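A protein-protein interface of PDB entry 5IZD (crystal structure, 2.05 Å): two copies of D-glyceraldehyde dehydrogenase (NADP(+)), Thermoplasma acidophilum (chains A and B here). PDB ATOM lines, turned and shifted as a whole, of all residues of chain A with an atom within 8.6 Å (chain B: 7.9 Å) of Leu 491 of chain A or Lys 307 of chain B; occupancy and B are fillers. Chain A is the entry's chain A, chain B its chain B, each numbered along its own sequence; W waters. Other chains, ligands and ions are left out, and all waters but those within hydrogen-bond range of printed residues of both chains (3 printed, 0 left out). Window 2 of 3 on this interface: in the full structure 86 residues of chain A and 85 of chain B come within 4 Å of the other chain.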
ATOM      1  N   THR A 486     -21.278 -22.255 -16.600  1.00  0.00           N
ATOM      2  CA  THR A 486     -22.560 -22.151 -17.303  1.00  0.00           C
ATOM      3  C   THR A 486     -22.799 -20.853 -18.052  1.00  0.00           C
ATOM      4  O   THR A 486     -23.892 -20.646 -18.570  1.00  0.00           O
ATOM      5  CB  THR A 486     -23.725 -22.354 -16.326  1.00  0.00           C
ATOM      6  OG1 THR A 486     -23.633 -21.390 -15.244  1.00  0.00           O
ATOM      7  CG2 THR A 486     -23.672 -23.798 -15.776  1.00  0.00           C
ATOM      8  N   VAL A 487     -21.798 -19.977 -18.083  1.00  0.00           N
ATOM      9  CA  VAL A 487     -21.864 -18.709 -18.785  1.00  0.00           C
ATOM     10  C   VAL A 487     -20.876 -18.810 -19.979  1.00  0.00           C
ATOM     11  O   VAL A 487     -19.683 -18.962 -19.794  1.00  0.00           O
ATOM     12  CB  VAL A 487     -21.518 -17.525 -17.835  1.00  0.00           C
ATOM     13  CG1 VAL A 487     -21.417 -16.231 -18.603  1.00  0.00           C
ATOM     14  CG2 VAL A 487     -22.529 -17.416 -16.680  1.00  0.00           C
ATOM     15  N   ARG A 488     -21.384 -18.709 -21.194  1.00  0.00           N
ATOM     16  CA  ARG A 488     -20.560 -18.900 -22.377  1.00  0.00           C
ATOM     17  C   ARG A 488     -19.581 -17.776 -22.528  1.00  0.00           C
ATOM     18  O   ARG A 488     -19.949 -16.588 -22.509  1.00  0.00           O
ATOM     19  CB  ARG A 488     -21.419 -18.981 -23.625  1.00  0.00           C
ATOM     20  CG  ARG A 488     -22.365 -20.167 -23.643  1.00  0.00           C
ATOM     21  CD  ARG A 488     -23.182 -20.194 -24.939  1.00  0.00           C
ATOM     22  NE  ARG A 488     -24.408 -19.366 -24.890  1.00  0.00           N
ATOM     23  CZ  ARG A 488     -24.656 -18.299 -25.655  1.00  0.00           C
ATOM     24  NH1 ARG A 488     -23.788 -17.852 -26.574  1.00  0.00           N
ATOM     25  NH2 ARG A 488     -25.803 -17.674 -25.550  1.00  0.00           N
ATOM     26  N   ASP A 489     -18.319 -18.148 -22.715  1.00  0.00           N
ATOM     27  CA  ASP A 489     -17.268 -17.124 -22.917  1.00  0.00           C
ATOM     28  C   ASP A 489     -17.399 -16.425 -24.261  1.00  0.00           C
ATOM     29  O   ASP A 489     -16.969 -15.263 -24.362  1.00  0.00           O
ATOM     30  CB  ASP A 489     -15.816 -17.615 -22.558  1.00  0.00           C
ATOM     31  CG  ASP A 489     -15.497 -17.429 -20.972  1.00  0.00           C
ATOM     32  OD1 ASP A 489     -16.122 -16.560 -20.246  1.00  0.00           O
ATOM     33  OD2 ASP A 489     -14.603 -18.155 -20.452  1.00  0.00           O
ATOM     34  N   ASP A 490     -18.084 -17.036 -25.232  1.00  0.00           N
ATOM     35  CA  ASP A 490     -18.385 -16.319 -26.493  1.00  0.00           C
ATOM     36  C   ASP A 490     -19.366 -15.108 -26.342  1.00  0.00           C
ATOM     37  O   ASP A 490     -19.441 -14.268 -27.246  1.00  0.00           O
ATOM     38  CB  ASP A 490     -18.797 -17.274 -27.651  1.00  0.00           C
ATOM     39  CG  ASP A 490     -20.182 -17.886 -27.470  1.00  0.00           C
ATOM     40  OD1 ASP A 490     -20.793 -17.787 -26.395  1.00  0.00           O
ATOM     41  OD2 ASP A 490     -20.678 -18.476 -28.432  1.00  0.00           O
ATOM     42  N   LEU A 491     -20.072 -14.992 -25.214  1.00  0.00           N
ATOM     43  CA  LEU A 491     -20.822 -13.745 -24.891  1.00  0.00           C
ATOM     44  C   LEU A 491     -19.933 -12.569 -24.562  1.00  0.00           C
ATOM     45  O   LEU A 491     -20.410 -11.452 -24.571  1.00  0.00           O
ATOM     46  CB  LEU A 491     -21.757 -13.935 -23.689  1.00  0.00           C
ATOM     47  CG  LEU A 491     -22.842 -14.973 -23.902  1.00  0.00           C
ATOM     48  CD1 LEU A 491     -23.430 -15.361 -22.566  1.00  0.00           C
ATOM     49  CD2 LEU A 491     -23.911 -14.443 -24.846  1.00  0.00           C
ATOM     50  N   PHE A 492     -18.669 -12.826 -24.230  1.00  0.00           N
ATOM     51  CA  PHE A 492     -17.706 -11.778 -23.885  1.00  0.00           C
ATOM     52  C   PHE A 492     -16.541 -11.641 -24.885  1.00  0.00           C
ATOM     53  O   PHE A 492     -15.602 -10.907 -24.619  1.00  0.00           O
ATOM     54  CB  PHE A 492     -17.239 -12.006 -22.435  1.00  0.00           C
ATOM     55  CG  PHE A 492     -18.359 -11.807 -21.434  1.00  0.00           C
ATOM     56  CD1 PHE A 492     -19.251 -12.825 -21.158  1.00  0.00           C
ATOM     57  CD2 PHE A 492     -18.583 -10.548 -20.872  1.00  0.00           C
ATOM     58  CE1 PHE A 492     -20.318 -12.617 -20.277  1.00  0.00           C
ATOM     59  CE2 PHE A 492     -19.637 -10.336 -19.981  1.00  0.00           C
ATOM     60  CZ  PHE A 492     -20.511 -11.372 -19.689  1.00  0.00           C
ATOM     61  N   GLN A 493     -16.666 -12.249 -26.057  1.00  0.00           N
ATOM     62  CA  GLN A 493     -15.618 -12.219 -27.099  1.00  0.00           C
ATOM     63  C   GLN A 493     -16.022 -11.402 -28.331  1.00  0.00           C
ATOM     64  O   GLN A 493     -17.217 -11.340 -28.672  1.00  0.00           O
ATOM     65  CB  GLN A 493     -15.267 -13.663 -27.531  1.00  0.00           C
ATOM     66  CG  GLN A 493     -14.295 -14.357 -26.582  1.00  0.00           C
ATOM     67  CD  GLN A 493     -13.033 -13.526 -26.334  1.00  0.00           C
ATOM     68  OE1 GLN A 493     -12.425 -12.978 -27.275  1.00  0.00           O
ATOM     69  NE2 GLN A 493     -12.643 -13.404 -25.069  1.00  0.00           N
ATOM     70  N   SER A 494     -15.021 -10.820 -29.008  1.00  0.00           N
ATOM     71  CA  SER A 494     -15.261  -9.916 -30.148  1.00  0.00           C
ATOM     72  C   SER A 494     -15.692 -10.647 -31.419  1.00  0.00           C
ATOM     73  O   SER A 494     -14.984 -11.539 -31.887  1.00  0.00           O
ATOM     74  CB  SER A 494     -14.037  -9.023 -30.406  1.00  0.00           C
ATOM     75  OG  SER A 494     -12.896  -9.757 -30.787  1.00  0.00           O
ATOM     76  N   ASP B 263     -16.619  -6.512 -16.882  1.00  0.00           N
ATOM     77  CA  ASP B 263     -16.840  -7.841 -17.509  1.00  0.00           C
ATOM     78  C   ASP B 263     -17.101  -8.887 -16.421  1.00  0.00           C
ATOM     79  O   ASP B 263     -18.069  -9.631 -16.501  1.00  0.00           O
ATOM     80  CB  ASP B 263     -15.665  -8.334 -18.368  1.00  0.00           C
ATOM     81  CG  ASP B 263     -15.584  -7.657 -19.737  1.00  0.00           C
ATOM     82  OD1 ASP B 263     -16.534  -6.942 -20.217  1.00  0.00           O
ATOM     83  OD2 ASP B 263     -14.503  -7.896 -20.340  1.00  0.00           O
ATOM     84  N   LYS B 267     -20.534 -11.047 -16.094  1.00  0.00           N
ATOM     85  CA  LYS B 267     -20.459 -12.500 -16.048  1.00  0.00           C
ATOM     86  C   LYS B 267     -21.138 -13.052 -14.809  1.00  0.00           C
ATOM     87  O   LYS B 267     -21.998 -13.891 -14.919  1.00  0.00           O
ATOM     88  CB  LYS B 267     -19.023 -13.031 -16.088  1.00  0.00           C
ATOM     89  CG  LYS B 267     -18.417 -13.001 -17.446  1.00  0.00           C
ATOM     90  CD  LYS B 267     -16.964 -13.430 -17.360  1.00  0.00           C
ATOM     91  CE  LYS B 267     -16.322 -13.386 -18.754  1.00  0.00           C
ATOM     92  NZ  LYS B 267     -14.849 -13.602 -18.554  1.00  0.00           N
ATOM     93  N   LEU B 270     -24.984 -12.563 -14.841  1.00  0.00           N
ATOM     94  CA  LEU B 270     -25.682 -13.577 -15.703  1.00  0.00           C
ATOM     95  C   LEU B 270     -25.843 -14.873 -14.952  1.00  0.00           C
ATOM     96  O   LEU B 270     -26.913 -15.439 -14.953  1.00  0.00           O
ATOM     97  CB  LEU B 270     -24.979 -13.860 -17.004  1.00  0.00           C
ATOM     98  CG  LEU B 270     -24.866 -12.694 -17.986  1.00  0.00           C
ATOM     99  CD1 LEU B 270     -24.044 -13.137 -19.187  1.00  0.00           C
ATOM    100  CD2 LEU B 270     -26.198 -12.133 -18.460  1.00  0.00           C
ATOM    101  N   ARG B 300     -25.276  -3.036 -21.339  1.00  0.00           N
ATOM    102  CA  ARG B 300     -24.652  -4.347 -21.567  1.00  0.00           C
ATOM    103  C   ARG B 300     -25.463  -5.478 -20.992  1.00  0.00           C
ATOM    104  O   ARG B 300     -25.516  -6.552 -21.600  1.00  0.00           O
ATOM    105  CB  ARG B 300     -23.213  -4.381 -21.033  1.00  0.00           C
ATOM    106  CG  ARG B 300     -22.310  -3.475 -21.850  1.00  0.00           C
ATOM    107  CD  ARG B 300     -20.877  -3.603 -21.398  1.00  0.00           C
ATOM    108  NE  ARG B 300     -20.441  -4.957 -21.686  1.00  0.00           N
ATOM    109  CZ  ARG B 300     -19.348  -5.553 -21.212  1.00  0.00           C
ATOM    110  NH1 ARG B 300     -19.130  -6.851 -21.538  1.00  0.00           N
ATOM    111  NH2 ARG B 300     -18.481  -4.910 -20.428  1.00  0.00           N
ATOM    112  N   PHE B 301     -26.065  -5.264 -19.816  1.00  0.00           N
ATOM    113  CA  PHE B 301     -26.817  -6.323 -19.164  1.00  0.00           C
ATOM    114  C   PHE B 301     -27.978  -6.746 -20.047  1.00  0.00           C
ATOM    115  O   PHE B 301     -28.241  -7.932 -20.226  1.00  0.00           O
ATOM    116  CB  PHE B 301     -27.290  -5.869 -17.767  1.00  0.00           C
ATOM    117  CG  PHE B 301     -28.063  -6.909 -16.979  1.00  0.00           C
ATOM    118  CD1 PHE B 301     -27.711  -8.240 -16.990  1.00  0.00           C
ATOM    119  CD2 PHE B 301     -29.092  -6.514 -16.163  1.00  0.00           C
ATOM    120  CE1 PHE B 301     -28.433  -9.160 -16.250  1.00  0.00           C
ATOM    121  CE2 PHE B 301     -29.802  -7.425 -15.399  1.00  0.00           C
ATOM    122  CZ  PHE B 301     -29.474  -8.764 -15.465  1.00  0.00           C
ATOM    123  N   VAL B 302     -28.650  -5.759 -20.616  1.00  0.00           N
ATOM    124  CA  VAL B 302     -29.781  -5.986 -21.499  1.00  0.00           C
ATOM    125  C   VAL B 302     -29.304  -6.698 -22.757  1.00  0.00           C
ATOM    126  O   VAL B 302     -29.959  -7.664 -23.169  1.00  0.00           O
ATOM    127  CB  VAL B 302     -30.493  -4.663 -21.880  1.00  0.00           C
ATOM    128  CG1 VAL B 302     -31.494  -4.865 -23.017  1.00  0.00           C
ATOM    129  CG2 VAL B 302     -31.188  -4.071 -20.670  1.00  0.00           C
ATOM    130  N   GLU B 303     -28.188  -6.234 -23.351  1.00  0.00           N
ATOM    131  CA  GLU B 303     -27.670  -6.835 -24.604  1.00  0.00           C
ATOM    132  C   GLU B 303     -27.305  -8.322 -24.409  1.00  0.00           C
ATOM    133  O   GLU B 303     -27.684  -9.146 -25.240  1.00  0.00           O
ATOM    134  CB  GLU B 303     -26.479  -6.035 -25.161  1.00  0.00           C
ATOM    135  CG  GLU B 303     -25.818  -6.597 -26.441  1.00  0.00           C
ATOM    136  CD  GLU B 303     -24.605  -5.767 -26.849  1.00  0.00           C
ATOM    137  OE1 GLU B 303     -23.582  -5.827 -26.092  1.00  0.00           O
ATOM    138  OE2 GLU B 303     -24.714  -5.026 -27.868  1.00  0.00           O
ATOM    139  N   LEU B 304     -26.640  -8.663 -23.302  1.00  0.00           N
ATOM    140  CA  LEU B 304     -26.337 -10.062 -22.985  1.00  0.00           C
ATOM    141  C   LEU B 304     -27.591 -10.891 -22.681  1.00  0.00           C
ATOM    142  O   LEU B 304     -27.698 -12.037 -23.121  1.00  0.00           O
ATOM    143  CB  LEU B 304     -25.347 -10.200 -21.813  1.00  0.00           C
ATOM    144  CG  LEU B 304     -23.948  -9.580 -21.985  1.00  0.00           C
ATOM    145  CD1 LEU B 304     -23.401  -9.126 -20.645  1.00  0.00           C
ATOM    146  CD2 LEU B 304     -22.981 -10.530 -22.693  1.00  0.00           C
ATOM    147  N   SER B 305     -28.550 -10.319 -21.946  1.00  0.00           N
ATOM    148  CA  SER B 305     -29.731 -11.082 -21.548  1.00  0.00           C
ATOM    149  C   SER B 305     -30.529 -11.510 -22.778  1.00  0.00           C
ATOM    150  O   SER B 305     -31.093 -12.604 -22.805  1.00  0.00           O
ATOM    151  CB  SER B 305     -30.596 -10.286 -20.546  1.00  0.00           C
ATOM    152  OG  SER B 305     -29.876 -10.040 -19.343  1.00  0.00           O
ATOM    153  N   ARG B 306     -30.572 -10.646 -23.799  1.00  0.00           N
ATOM    154  CA  ARG B 306     -31.238 -10.957 -25.055  1.00  0.00           C
ATOM    155  C   ARG B 306     -30.598 -12.177 -25.796  1.00  0.00           C
ATOM    156  O   ARG B 306     -31.246 -12.807 -26.584  1.00  0.00           O
ATOM    157  CB  ARG B 306     -31.290  -9.699 -25.964  1.00  0.00           C
ATOM    158  CG  ARG B 306     -31.999  -9.873 -27.314  1.00  0.00           C
ATOM    159  CD  ARG B 306     -31.957  -8.657 -28.247  1.00  0.00           C
ATOM    160  NE  ARG B 306     -32.630  -7.519 -27.614  1.00  0.00           N
ATOM    161  CZ  ARG B 306     -32.043  -6.449 -27.076  1.00  0.00           C
ATOM    162  NH1 ARG B 306     -32.816  -5.501 -26.522  1.00  0.00           N
ATOM    163  NH2 ARG B 306     -30.717  -6.296 -27.097  1.00  0.00           N
ATOM    164  N   LYS B 307     -29.344 -12.503 -25.532  1.00  0.00           N
ATOM    165  CA  LYS B 307     -28.673 -13.604 -26.234  1.00  0.00           C
ATOM    166  C   LYS B 307     -28.795 -14.914 -25.522  1.00  0.00           C
ATOM    167  O   LYS B 307     -28.242 -15.892 -25.959  1.00  0.00           O
ATOM    168  CB  LYS B 307     -27.204 -13.279 -26.410  1.00  0.00           C
ATOM    169  CG  LYS B 307     -27.002 -12.024 -27.217  1.00  0.00           C
ATOM    170  CD  LYS B 307     -25.538 -11.625 -27.376  1.00  0.00           C
ATOM    171  CE  LYS B 307     -25.507 -10.594 -28.479  1.00  0.00           C
ATOM    172  NZ  LYS B 307     -24.249  -9.833 -28.470  1.00  0.00           N
ATOM    173  N   LEU B 308     -29.513 -14.954 -24.416  1.00  0.00           N
ATOM    174  CA  LEU B 308     -29.685 -16.208 -23.717  1.00  0.00           C
ATOM    175  C   LEU B 308     -30.753 -17.074 -24.408  1.00  0.00           C
ATOM    176  O   LEU B 308     -31.889 -16.639 -24.563  1.00  0.00           O
ATOM    177  CB  LEU B 308     -29.998 -15.954 -22.246  1.00  0.00           C
ATOM    178  CG  LEU B 308     -28.875 -15.256 -21.463  1.00  0.00           C
ATOM    179  CD1 LEU B 308     -29.332 -14.987 -20.037  1.00  0.00           C
ATOM    180  CD2 LEU B 308     -27.585 -16.060 -21.392  1.00  0.00           C
ATOM    181  N   ALA B 309     -30.373 -18.281 -24.836  1.00  0.00           N
ATOM    182  CA  ALA B 309     -31.339 -19.234 -25.413  1.00  0.00           C
ATOM    183  C   ALA B 309     -32.121 -20.044 -24.344  1.00  0.00           C
ATOM    184  O   ALA B 309     -31.562 -20.527 -23.371  1.00  0.00           O
ATOM    185  CB  ALA B 309     -30.681 -20.162 -26.445  1.00  0.00           C
ATOM    186  N   LEU B 310     -33.426 -20.140 -24.564  1.00  0.00           N
ATOM    187  CA  LEU B 310     -34.380 -20.831 -23.710  1.00  0.00           C
ATOM    188  C   LEU B 310     -34.953 -21.984 -24.487  1.00  0.00           C
ATOM    189  O   LEU B 310     -35.279 -21.818 -25.639  1.00  0.00           O
ATOM    190  CB  LEU B 310     -35.547 -19.900 -23.344  1.00  0.00           C
ATOM    191  CG  LEU B 310     -35.327 -19.049 -22.107  1.00  0.00           C
ATOM    192  CD1 LEU B 310     -34.248 -18.018 -22.402  1.00  0.00           C
ATOM    193  CD2 LEU B 310     -36.603 -18.346 -21.701  1.00  0.00           C
ATOM    194  N   ASP B 317     -29.350 -21.943 -22.798  1.00  0.00           N
ATOM    195  CA  ASP B 317     -28.680 -21.241 -21.660  1.00  0.00           C
ATOM    196  C   ASP B 317     -29.515 -21.241 -20.376  1.00  0.00           C
ATOM    197  O   ASP B 317     -28.973 -21.230 -19.274  1.00  0.00           O
ATOM    198  CB  ASP B 317     -28.361 -19.791 -22.010  1.00  0.00           C
ATOM    199  CG  ASP B 317     -27.434 -19.680 -23.188  1.00  0.00           C
ATOM    200  OD1 ASP B 317     -26.241 -20.076 -23.073  1.00  0.00           O
ATOM    201  OD2 ASP B 317     -27.881 -19.158 -24.220  1.00  0.00           O
ATOM    202  N   PHE B 346     -36.316  -5.030 -20.570  1.00  0.00           N
ATOM    203  CA  PHE B 346     -36.284  -6.196 -21.462  1.00  0.00           C
ATOM    204  C   PHE B 346     -37.173  -7.298 -20.902  1.00  0.00           C
ATOM    205  O   PHE B 346     -37.260  -7.466 -19.714  1.00  0.00           O
ATOM    206  CB  PHE B 346     -34.845  -6.733 -21.659  1.00  0.00           C
ATOM    207  CG  PHE B 346     -34.779  -7.926 -22.576  1.00  0.00           C
ATOM    208  CD1 PHE B 346     -34.890  -7.765 -23.936  1.00  0.00           C
ATOM    209  CD2 PHE B 346     -34.652  -9.218 -22.072  1.00  0.00           C
ATOM    210  CE1 PHE B 346     -34.874  -8.868 -24.780  1.00  0.00           C
ATOM    211  CE2 PHE B 346     -34.653 -10.328 -22.902  1.00  0.00           C
ATOM    212  CZ  PHE B 346     -34.780 -10.149 -24.252  1.00  0.00           C
ATOM    213  N   PRO B 365     -35.904 -13.645 -19.545  1.00  0.00           N
ATOM    214  CA  PRO B 365     -35.126 -12.728 -18.724  1.00  0.00           C
ATOM    215  C   PRO B 365     -35.822 -11.401 -18.710  1.00  0.00           C
ATOM    216  O   PRO B 365     -36.230 -10.928 -19.757  1.00  0.00           O
ATOM    217  CB  PRO B 365     -33.815 -12.609 -19.517  1.00  0.00           C
ATOM    218  CG  PRO B 365     -33.656 -13.967 -20.126  1.00  0.00           C
ATOM    219  CD  PRO B 365     -35.043 -14.327 -20.542  1.00  0.00           C
HETATM  220  O   HOH W   1     -24.820 -21.926 -20.933  1.00  0.00           O
HETATM  221  O   HOH W   2     -24.400 -18.581 -21.269  1.00  0.00           O
HETATM  222  O   HOH W   3     -20.225  -8.573 -23.689  1.00  0.00           O
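CG2 of Val 487 of chain A touches O of Lys 267 of chain B, 3.98 Å away. O of Leu 491 of chain A touches CD2 of Leu 304 of chain B, at 3.3 Å. Leu 491 of chain A touches Lys 307 of chain B (CD2 to CB, 3.8 Å). Asp 263 of chain B touches Phe 492 of chain A. CE1 of Phe 492 of chain A touches CG of Lys 267 of chain B, at 3.4 Å. Phe 492 of chain A touches Leu 270 of chain B. Phe 492 of chain A touches Arg 300 of chain B. Phe 492 of chain A touches Leu 304 of chain B.
Water W1 lies within hydrogen-bond range of the backbone carbonyl oxygen of Thr 486 of chain A (2.8 Å) and the side-chain carboxylate of Asp 317 of chain B (3.2 Å). Water W3 bridges NH1 of Arg 300 of chain B (3.0 Å) and O of Leu 491 of chain A (3.0 Å). Water W2 lies within hydrogen-bond range of the side-chain carboxylate (OD1) of Asp 317 of chain B, the backbone NH (N) of Arg 488 of chain A and the backbone carbonyl oxygen (O) of Thr 486 of chain A.
No position is printed for both chains.
Of the 17 printed residues of chain B, 7 touch a printed residue of chain A. Hydrophobic or aromatic side chains of chain B within 4 Å of the printed part of chain A: Leu 270 and Leu 304. Of the 9 printed residues of chain A, 5 touch a printed residue of chain B. Printed residues of chain A that touch a printed residue of chain B: Val 487, Arg 488, Asp 489, Leu 491 and Phe 492. Among the printed residues, 11 pairs touch across the chains. Among the printed residues, Asp or Glu carboxylates within 4 Å of a Lys or Arg side-chain nitrogen of the other chain: Arg 488 of chain A with Asp 317 of chain B (2.7 Å) and Asp 489 of chain A with Lys 267 of chain B (3.6 Å).
The guanidinium group of Arg 488 of chain A lies within salt-bridge range of the side-chain carboxylate of Asp 490 of chain A, at 3.0 Å. The side-chain carboxylate (OD1) of Asp 263 of chain B is in salt-bridge range of the guanidinium group (NH2) of Arg 300 of chain B, 2.8 Å away. The backbone NH of Asp 317 of chain B is in hydrogen-bond range of the backbone carbonyl oxygen of Ala 309 of chain B (2.7 Å).
The backbone carbonyl oxygen of Lys 307 of chain B is in hydrogen-bond range of the guanidinium group of Arg 488 of chain A (3.0 Å). NE of Arg 488 of chain A is in salt-bridge range of OD1 of Asp 317 of chain B (2.7 Å). The side-chain amino group (NZ) of Lys 267 of chain B lies within salt-bridge range of the side-chain carboxylate (OD1) of Asp 489 of chain A (3.6 Å).
Leu 491 of chain A touches two residues of chain B. Lys 307 of chain B touches two residues of chain A. Printed residues of chain A within 4 Å of Asp 317 of chain B: Arg 488. Of the printed residues of chain B, Phe 492 of chain A touches Asp 263, Lys 267, Leu 270, Arg 300 and Leu 304. Printed residues of chain A within 4 Å of Lys 267 of chain B: Val 487, Asp 489 and Phe 492. Of the printed residues of chain A, Leu 270 of chain B touches Phe 492. The nearest residue of chain B that does not touch Leu 491 of chain A is Leu 270 of chain B (4.1 Å). The nearest residue of chain A that does not touch Lys 307 of chain B is Asp 490 of chain A (6.6 Å). The nearest printed residue of chain A that does not touch Arg 300 of chain B is Leu 491 of chain A (5.7 Å).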
